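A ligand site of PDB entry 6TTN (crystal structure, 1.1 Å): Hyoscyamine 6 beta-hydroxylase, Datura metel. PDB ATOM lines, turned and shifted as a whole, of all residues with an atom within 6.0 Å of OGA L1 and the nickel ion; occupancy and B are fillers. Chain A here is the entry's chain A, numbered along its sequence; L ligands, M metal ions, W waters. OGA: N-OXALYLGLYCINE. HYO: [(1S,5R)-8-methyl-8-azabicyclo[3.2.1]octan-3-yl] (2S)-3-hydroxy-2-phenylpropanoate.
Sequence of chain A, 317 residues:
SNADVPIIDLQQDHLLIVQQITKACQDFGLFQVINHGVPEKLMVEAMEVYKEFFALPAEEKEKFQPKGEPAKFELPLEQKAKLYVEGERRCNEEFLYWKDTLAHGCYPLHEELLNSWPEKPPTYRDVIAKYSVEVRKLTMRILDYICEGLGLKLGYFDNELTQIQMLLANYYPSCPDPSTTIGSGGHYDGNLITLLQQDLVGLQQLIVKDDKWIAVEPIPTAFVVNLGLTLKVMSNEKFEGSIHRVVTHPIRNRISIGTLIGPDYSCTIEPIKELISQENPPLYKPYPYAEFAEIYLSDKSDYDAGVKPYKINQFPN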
ATOM      1  N   GLU A  86      -9.082 -29.359 -12.525  1.00  0.00           N
ATOM      2  CA  GLU A  86      -9.180 -29.702 -11.111  1.00  0.00           C
ATOM      3  C   GLU A  86      -9.659 -31.127 -11.006  1.00  0.00           C
ATOM      4  O   GLU A  86     -10.726 -31.449 -11.528  1.00  0.00           O
ATOM      5  CB  GLU A  86     -10.182 -28.761 -10.425  1.00  0.00           C
ATOM      6  CG  GLU A  86     -10.156 -28.833  -8.892  1.00  0.00           C
ATOM      7  CD  GLU A  86     -11.110 -27.888  -8.183  1.00  0.00           C
ATOM      8  OE1 GLU A  86     -11.950 -27.268  -8.843  1.00  0.00           O
ATOM      9  OE2 GLU A  86     -11.001 -27.743  -6.950  1.00  0.00           O
ATOM     10  N   LYS A  99     -13.756 -31.397 -15.787  1.00  0.00           N
ATOM     11  CA  LYS A  99     -14.160 -30.021 -15.549  1.00  0.00           C
ATOM     12  C   LYS A  99     -13.102 -29.055 -16.062  1.00  0.00           C
ATOM     13  O   LYS A  99     -11.939 -29.117 -15.662  1.00  0.00           O
ATOM     14  CB  LYS A  99     -14.374 -29.746 -14.050  1.00  0.00           C
ATOM     15  CG  LYS A  99     -14.833 -28.292 -13.760  1.00  0.00           C
ATOM     16  CD  LYS A  99     -15.212 -28.059 -12.289  1.00  0.00           C
ATOM     17  CE  LYS A  99     -14.054 -28.168 -11.293  1.00  0.00           C
ATOM     18  NZ  LYS A  99     -13.223 -26.953 -11.222  1.00  0.00           N
ATOM     19  N   LEU A 168     -15.914 -18.174 -11.548  1.00  0.00           N
ATOM     20  CA  LEU A 168     -15.498 -19.500 -12.003  1.00  0.00           C
ATOM     21  C   LEU A 168     -16.606 -20.011 -12.913  1.00  0.00           C
ATOM     22  O   LEU A 168     -17.686 -20.376 -12.429  1.00  0.00           O
ATOM     23  CB  LEU A 168     -15.282 -20.482 -10.855  1.00  0.00           C
ATOM     24  CG  LEU A 168     -13.918 -20.452 -10.147  1.00  0.00           C
ATOM     25  CD1 LEU A 168     -13.580 -19.111  -9.554  1.00  0.00           C
ATOM     26  CD2 LEU A 168     -13.811 -21.544  -9.109  1.00  0.00           C
ATOM     27  N   ASN A 170     -17.711 -22.941 -15.225  1.00  0.00           N
ATOM     28  CA  ASN A 170     -17.342 -24.345 -15.291  1.00  0.00           C
ATOM     29  C   ASN A 170     -18.029 -25.028 -16.462  1.00  0.00           C
ATOM     30  O   ASN A 170     -19.224 -24.854 -16.678  1.00  0.00           O
ATOM     31  CB  ASN A 170     -17.823 -25.046 -14.022  1.00  0.00           C
ATOM     32  CG  ASN A 170     -17.366 -24.319 -12.792  1.00  0.00           C
ATOM     33  OD1 ASN A 170     -16.170 -24.162 -12.561  1.00  0.00           O
ATOM     34  ND2 ASN A 170     -18.326 -23.810 -12.031  1.00  0.00           N
ATOM     35  N   TYR A 172     -18.514 -28.905 -17.933  1.00  0.00           N
ATOM     36  CA  TYR A 172     -18.457 -30.334 -17.569  1.00  0.00           C
ATOM     37  C   TYR A 172     -18.792 -31.129 -18.816  1.00  0.00           C
ATOM     38  O   TYR A 172     -19.963 -31.255 -19.173  1.00  0.00           O
ATOM     39  CB  TYR A 172     -19.477 -30.646 -16.470  1.00  0.00           C
ATOM     40  CG  TYR A 172     -19.257 -29.863 -15.196  1.00  0.00           C
ATOM     41  CD1 TYR A 172     -18.422 -30.351 -14.214  1.00  0.00           C
ATOM     42  CD2 TYR A 172     -19.956 -28.693 -14.956  1.00  0.00           C
ATOM     43  CE1 TYR A 172     -18.210 -29.634 -13.031  1.00  0.00           C
ATOM     44  CE2 TYR A 172     -19.775 -27.966 -13.769  1.00  0.00           C
ATOM     45  CZ  TYR A 172     -18.924 -28.461 -12.801  1.00  0.00           C
ATOM     46  OH  TYR A 172     -18.699 -27.792 -11.626  1.00  0.00           O
ATOM     47  N   HIS A 187     -17.108 -30.799  -1.566  1.00  0.00           N
ATOM     48  CA  HIS A 187     -16.259 -29.781  -0.981  1.00  0.00           C
ATOM     49  C   HIS A 187     -17.124 -28.732  -0.306  1.00  0.00           C
ATOM     50  O   HIS A 187     -18.286 -28.528  -0.660  1.00  0.00           O
ATOM     51  CB  HIS A 187     -15.374 -29.088  -2.046  1.00  0.00           C
ATOM     52  CG  HIS A 187     -16.154 -28.368  -3.108  1.00  0.00           C
ATOM     53  ND1 HIS A 187     -16.695 -28.999  -4.204  1.00  0.00           N
ATOM     54  CD2 HIS A 187     -16.528 -27.076  -3.227  1.00  0.00           C
ATOM     55  CE1 HIS A 187     -17.391 -28.134  -4.926  1.00  0.00           C
ATOM     56  NE2 HIS A 187     -17.276 -26.938  -4.360  1.00  0.00           N
ATOM     57  N   TYR A 188     -16.526 -28.046   0.673  1.00  0.00           N
ATOM     58  CA  TYR A 188     -16.954 -26.679   0.982  1.00  0.00           C
ATOM     59  C   TYR A 188     -16.255 -25.734   0.007  1.00  0.00           C
ATOM     60  O   TYR A 188     -15.109 -26.002  -0.387  1.00  0.00           O
ATOM     61  CB  TYR A 188     -16.443 -26.213   2.345  1.00  0.00           C
ATOM     62  CG  TYR A 188     -16.966 -26.862   3.602  1.00  0.00           C
ATOM     63  CD1 TYR A 188     -18.165 -26.469   4.164  1.00  0.00           C
ATOM     64  CD2 TYR A 188     -16.213 -27.818   4.267  1.00  0.00           C
ATOM     65  CE1 TYR A 188     -18.603 -27.019   5.342  1.00  0.00           C
ATOM     66  CE2 TYR A 188     -16.643 -28.371   5.433  1.00  0.00           C
ATOM     67  CZ  TYR A 188     -17.842 -27.974   5.986  1.00  0.00           C
ATOM     68  OH  TYR A 188     -18.298 -28.508   7.192  1.00  0.00           O
ATOM     69  N   ASP A 189     -16.906 -24.628  -0.361  1.00  0.00           N
ATOM     70  CA  ASP A 189     -16.162 -23.524  -0.949  1.00  0.00           C
ATOM     71  C   ASP A 189     -15.406 -22.854   0.185  1.00  0.00           C
ATOM     72  O   ASP A 189     -15.937 -22.666   1.271  1.00  0.00           O
ATOM     73  CB  ASP A 189     -17.108 -22.508  -1.601  1.00  0.00           C
ATOM     74  CG  ASP A 189     -17.834 -23.029  -2.827  1.00  0.00           C
ATOM     75  OD1 ASP A 189     -17.526 -24.155  -3.320  1.00  0.00           O
ATOM     76  OD2 ASP A 189     -18.706 -22.272  -3.324  1.00  0.00           O
ATOM     77  N   THR A 194     -20.841 -17.840  -1.922  1.00  0.00           N
ATOM     78  CA  THR A 194     -20.848 -18.082  -3.355  1.00  0.00           C
ATOM     79  C   THR A 194     -22.261 -18.020  -3.886  1.00  0.00           C
ATOM     80  O   THR A 194     -23.194 -18.534  -3.267  1.00  0.00           O
ATOM     81  CB  THR A 194     -20.276 -19.472  -3.630  1.00  0.00           C
ATOM     82  OG1 THR A 194     -18.941 -19.529  -3.119  1.00  0.00           O
ATOM     83  CG2 THR A 194     -20.323 -19.834  -5.122  1.00  0.00           C
ATOM     84  N   LEU A 196     -24.265 -19.147  -7.418  1.00  0.00           N
ATOM     85  CA  LEU A 196     -24.072 -20.045  -8.542  1.00  0.00           C
ATOM     86  C   LEU A 196     -25.317 -20.029  -9.436  1.00  0.00           C
ATOM     87  O   LEU A 196     -26.441 -20.205  -8.962  1.00  0.00           O
ATOM     88  CB  LEU A 196     -23.805 -21.450  -8.027  1.00  0.00           C
ATOM     89  CG  LEU A 196     -23.511 -22.404  -9.185  1.00  0.00           C
ATOM     90  CD1 LEU A 196     -22.073 -22.603  -9.473  1.00  0.00           C
ATOM     91  CD2 LEU A 196     -24.327 -23.663  -9.176  1.00  0.00           C
ATOM     92  N   GLN A 198     -27.103 -21.944 -12.572  1.00  0.00           N
ATOM     93  CA  GLN A 198     -27.150 -23.225 -13.269  1.00  0.00           C
ATOM     94  C   GLN A 198     -28.462 -23.360 -14.019  1.00  0.00           C
ATOM     95  O   GLN A 198     -29.469 -22.757 -13.663  1.00  0.00           O
ATOM     96  CB  GLN A 198     -26.999 -24.402 -12.307  1.00  0.00           C
ATOM     97  CG  GLN A 198     -28.046 -24.427 -11.223  1.00  0.00           C
ATOM     98  CD  GLN A 198     -28.205 -25.723 -10.483  1.00  0.00           C
ATOM     99  OE1 GLN A 198     -27.526 -26.706 -10.777  1.00  0.00           O
ATOM    100  NE2 GLN A 198     -29.092 -25.723  -9.517  1.00  0.00           N
ATOM    101  N   GLY A 202     -27.313 -31.483 -11.744  1.00  0.00           N
ATOM    102  CA  GLY A 202     -25.965 -31.932 -11.498  1.00  0.00           C
ATOM    103  C   GLY A 202     -25.444 -31.546 -10.124  1.00  0.00           C
ATOM    104  O   GLY A 202     -24.549 -32.214  -9.590  1.00  0.00           O
ATOM    105  N   LEU A 203     -25.951 -30.473  -9.534  1.00  0.00           N
ATOM    106  CA  LEU A 203     -25.490 -30.042  -8.217  1.00  0.00           C
ATOM    107  C   LEU A 203     -26.234 -30.792  -7.131  1.00  0.00           C
ATOM    108  O   LEU A 203     -27.463 -30.884  -7.152  1.00  0.00           O
ATOM    109  CB  LEU A 203     -25.718 -28.543  -8.069  1.00  0.00           C
ATOM    110  CG  LEU A 203     -25.314 -27.894  -6.740  1.00  0.00           C
ATOM    111  CD1 LEU A 203     -23.805 -28.020  -6.515  1.00  0.00           C
ATOM    112  CD2 LEU A 203     -25.716 -26.422  -6.744  1.00  0.00           C
ATOM    113  N   ASN A 226     -24.503 -20.394  -1.476  1.00  0.00           N
ATOM    114  CA  ASN A 226     -23.928 -21.313  -0.506  1.00  0.00           C
ATOM    115  C   ASN A 226     -22.882 -20.620   0.348  1.00  0.00           C
ATOM    116  O   ASN A 226     -22.114 -19.763  -0.113  1.00  0.00           O
ATOM    117  CB  ASN A 226     -23.431 -22.597  -1.094  1.00  0.00           C
ATOM    118  CG  ASN A 226     -22.317 -22.382  -2.016  1.00  0.00           C
ATOM    119  OD1 ASN A 226     -22.541 -22.115  -3.224  1.00  0.00           O
ATOM    120  ND2 ASN A 226     -21.069 -22.590  -1.523  1.00  0.00           N
ATOM    121  N   HIS A 244     -21.043 -29.596  -0.928  1.00  0.00           N
ATOM    122  CA  HIS A 244     -21.793 -29.872  -2.141  1.00  0.00           C
ATOM    123  C   HIS A 244     -20.878 -30.538  -3.159  1.00  0.00           C
ATOM    124  O   HIS A 244     -19.657 -30.559  -3.011  1.00  0.00           O
ATOM    125  CB  HIS A 244     -22.465 -28.588  -2.674  1.00  0.00           C
ATOM    126  CG  HIS A 244     -21.488 -27.456  -2.863  1.00  0.00           C
ATOM    127  ND1 HIS A 244     -21.121 -26.591  -1.857  1.00  0.00           N
ATOM    128  CD2 HIS A 244     -20.734 -27.092  -3.920  1.00  0.00           C
ATOM    129  CE1 HIS A 244     -20.215 -25.754  -2.314  1.00  0.00           C
ATOM    130  NE2 HIS A 244     -19.941 -26.042  -3.570  1.00  0.00           N
ATOM    131  N   ARG A 245     -21.479 -31.115  -4.201  1.00  0.00           N
ATOM    132  CA  ARG A 245     -20.729 -31.836  -5.220  1.00  0.00           C
ATOM    133  C   ARG A 245     -21.463 -31.726  -6.547  1.00  0.00           C
ATOM    134  O   ARG A 245     -22.645 -31.371  -6.593  1.00  0.00           O
ATOM    135  CB  ARG A 245     -20.530 -33.314  -4.853  1.00  0.00           C
ATOM    136  CG  ARG A 245     -21.780 -34.179  -4.968  1.00  0.00           C
ATOM    137  CD  ARG A 245     -21.530 -35.605  -4.505  1.00  0.00           C
ATOM    138  NE  ARG A 245     -22.739 -36.418  -4.696  1.00  0.00           N
ATOM    139  CZ  ARG A 245     -22.875 -37.656  -4.245  1.00  0.00           C
ATOM    140  NH1 ARG A 245     -21.884 -38.223  -3.585  1.00  0.00           N
ATOM    141  NH2 ARG A 245     -24.009 -38.314  -4.471  1.00  0.00           N
ATOM    142  N   VAL A 246     -20.743 -32.058  -7.625  1.00  0.00           N
ATOM    143  CA  VAL A 246     -21.325 -32.016  -8.958  1.00  0.00           C
ATOM    144  C   VAL A 246     -21.264 -33.396  -9.597  1.00  0.00           C
ATOM    145  O   VAL A 246     -20.213 -34.040  -9.603  1.00  0.00           O
ATOM    146  CB  VAL A 246     -20.603 -30.997  -9.860  1.00  0.00           C
ATOM    147  CG1 VAL A 246     -21.152 -31.011 -11.291  1.00  0.00           C
ATOM    148  CG2 VAL A 246     -20.709 -29.605  -9.227  1.00  0.00           C
ATOM    149  N   ARG A 254     -22.675 -29.597 -19.361  1.00  0.00           N
ATOM    150  CA  ARG A 254     -23.251 -28.633 -18.427  1.00  0.00           C
ATOM    151  C   ARG A 254     -22.303 -27.472 -18.162  1.00  0.00           C
ATOM    152  O   ARG A 254     -21.103 -27.671 -17.999  1.00  0.00           O
ATOM    153  CB  ARG A 254     -23.557 -29.380 -17.133  1.00  0.00           C
ATOM    154  CG  ARG A 254     -24.150 -28.529 -16.019  1.00  0.00           C
ATOM    155  CD  ARG A 254     -24.639 -29.404 -14.874  1.00  0.00           C
ATOM    156  NE  ARG A 254     -25.151 -28.633 -13.759  1.00  0.00           N
ATOM    157  CZ  ARG A 254     -24.400 -28.071 -12.819  1.00  0.00           C
ATOM    158  NH1 ARG A 254     -23.096 -28.222 -12.853  1.00  0.00           N
ATOM    159  NH2 ARG A 254     -24.934 -27.341 -11.861  1.00  0.00           N
ATOM    160  N   SER A 256     -21.937 -24.054 -15.550  1.00  0.00           N
ATOM    161  CA  SER A 256     -22.413 -23.297 -14.408  1.00  0.00           C
ATOM    162  C   SER A 256     -21.524 -22.076 -14.237  1.00  0.00           C
ATOM    163  O   SER A 256     -20.362 -22.058 -14.667  1.00  0.00           O
ATOM    164  CB  SER A 256     -22.414 -24.132 -13.148  1.00  0.00           C
ATOM    165  OG  SER A 256     -21.103 -24.488 -12.822  1.00  0.00           O
ATOM    166  N   LEU A 260     -17.568 -16.354  -6.483  1.00  0.00           N
ATOM    167  CA  LEU A 260     -17.030 -16.763  -5.190  1.00  0.00           C
ATOM    168  C   LEU A 260     -16.411 -15.523  -4.550  1.00  0.00           C
ATOM    169  O   LEU A 260     -15.357 -15.035  -4.985  1.00  0.00           O
ATOM    170  CB  LEU A 260     -15.968 -17.848  -5.341  1.00  0.00           C
ATOM    171  CG  LEU A 260     -16.477 -19.269  -5.622  1.00  0.00           C
ATOM    172  CD1 LEU A 260     -17.091 -19.399  -7.035  1.00  0.00           C
ATOM    173  CD2 LEU A 260     -15.354 -20.245  -5.427  1.00  0.00           C
HETATM  174  C1  OGA L   1     -17.732 -25.007  -7.466  1.00  0.00           C
HETATM  175  C2  OGA L   1     -19.062 -25.674  -7.470  1.00  0.00           C
HETATM  176  C4  OGA L   1     -21.109 -26.280  -8.617  1.00  0.00           C
HETATM  177  C5  OGA L   1     -21.588 -26.475 -10.012  1.00  0.00           C
HETATM  178  O1  OGA L   1     -17.240 -24.721  -6.390  1.00  0.00           O
HETATM  179  O2  OGA L   1     -17.197 -24.734  -8.626  1.00  0.00           O
HETATM  180  O2' OGA L   1     -19.472 -26.169  -6.421  1.00  0.00           O
HETATM  181  O3  OGA L   1     -20.840 -26.334 -10.975  1.00  0.00           O
HETATM  182  N1  OGA L   1     -19.782 -25.707  -8.607  1.00  0.00           N
HETATM  183  O4  OGA L   1     -22.837 -26.779 -10.107  1.00  0.00           O
HETATM  184  C10 HYO L   2     -11.714 -24.143  -6.985  1.00  0.00           C
HETATM  185  C13 HYO L   2     -10.995 -21.689  -5.157  1.00  0.00           C
HETATM  186  C15 HYO L   2     -10.781 -20.386  -3.114  1.00  0.00           C
HETATM  187  C17 HYO L   2     -11.493 -20.126  -1.871  1.00  0.00           C
HETATM  188  C20 HYO L   2      -8.585 -20.279  -1.876  1.00  0.00           C
HETATM  189  C21 HYO L   2      -9.313 -20.008  -0.629  1.00  0.00           C
HETATM  190  C05 HYO L   2     -13.097 -25.603  -4.991  1.00  0.00           C
HETATM  191  C06 HYO L   2     -13.121 -24.695  -7.019  1.00  0.00           C
HETATM  192  C07 HYO L   2     -14.101 -24.417  -4.843  1.00  0.00           C
HETATM  193  C08 HYO L   2     -14.090 -23.803  -6.180  1.00  0.00           C
HETATM  194  C09 HYO L   2     -11.680 -25.217  -4.636  1.00  0.00           C
HETATM  195  C11 HYO L   2     -11.160 -23.970  -5.491  1.00  0.00           C
HETATM  196  C12 HYO L   2     -14.416 -26.676  -6.666  1.00  0.00           C
HETATM  197  C14 HYO L   2     -11.545 -20.517  -4.388  1.00  0.00           C
HETATM  198  C16 HYO L   2     -11.424 -19.184  -5.178  1.00  0.00           C
HETATM  199  C18 HYO L   2      -9.317 -20.444  -3.131  1.00  0.00           C
HETATM  200  C19 HYO L   2     -10.771 -19.939  -0.618  1.00  0.00           C
HETATM  201  N04 HYO L   2     -13.233 -25.931  -6.352  1.00  0.00           N
HETATM  202  O01 HYO L   2     -11.630 -22.859  -4.864  1.00  0.00           O
HETATM  203  O02 HYO L   2     -10.096 -21.622  -5.978  1.00  0.00           O
HETATM  204  O03 HYO L   2     -11.895 -18.083  -4.393  1.00  0.00           O
HETATM  205 NI    NI M   1     -18.477 -25.279  -4.810  1.00  0.00          NI
HETATM  206  O   HOH W   1     -16.962 -27.779  -9.458  1.00  0.00           O
HETATM  207  O   HOH W   2     -18.186 -22.088  -9.832  1.00  0.00           O
HETATM  208  O   HOH W   3     -19.673 -23.602  -5.381  1.00  0.00           O
HETATM  209  O   HOH W   4     -14.990 -24.829 -10.162  1.00  0.00           O
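The side-chain carboxylate (OE2) of Glu 86 is in salt-bridge range of a nitrogen (N04) of HYO L2, 2.9 Å away. OH of Tyr 172 sits at hydrogen-bond distance from O3 of OGA L1 (2.7 Å). OG of Ser 256 is in hydrogen-bond range of O3 of OGA L1, 2.6 Å away. The guanidinium group (NH2) of Arg 254 is in salt-bridge range of an oxygen (O4) of OGA L1.
The backbone carbonyl oxygen (O) of Arg 254 is in hydrogen-bond range of the backbone NH (N) of Tyr 172, at 2.9 Å. OD2 of Asp 189 sits at hydrogen-bond distance from ND2 of Asn 226, at 3.0 Å. The side-chain carboxylate (OD2) of Asp 189 lies within hydrogen-bond range of the side-chain hydroxyl (OG1) of Thr 194, 2.8 Å away. N of Asn 170 lies within hydrogen-bond range of O of Ser 256, at 2.8 Å. The side-chain amide oxygen (OE1) of Gln 198 is in hydrogen-bond range of the guanidinium group (NH2) of Arg 254.
Asn 170 touches OGA L1. Leu 196 touches OGA L1. Leu 203 touches OGA L1 (CD1 to C4, 3.8 Å). Val 246 touches OGA L1 (CG2 to C5, 3.3 Å). The nearest printed residue that does not touch OGA L1 is Leu 168 (4.7 Å).
Of the 20 residues printed, 3 come within 4 Å of the nickel ion. The nearest printed residue that does not touch the nickel ion is Asn 226 (5.0 Å).
NE2 of His 244 is bound to the nickel ion. O1 of OGA L1 binds the nickel ion. The nickel ion is bound by O2' of OGA L1 (2.1 Å). OD1 of Asp 189 binds the nickel ion. NE2 of His 187 binds the nickel ion (2.1 Å). The nickel ion is bound by water W3 (2.1 Å).
Water W4 lies within hydrogen-bond range of an oxygen (O2) of OGA L1, the side-chain amide oxygen (OD1) of Asn 170 and the side-chain amino group (NZ) of Lys 99. Water W2 lies within hydrogen-bond range of the side-chain amide nitrogen of Asn 170 (2.8 Å), an oxygen (O2) of OGA L1 (3.1 Å) and the backbone carbonyl oxygen of Leu 168 (3.2 Å). Water W1 bridges the side-chain hydroxyl (OH) of Tyr 172 (2.8 Å) and an oxygen (O2) of OGA L1 (3.2 Å).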
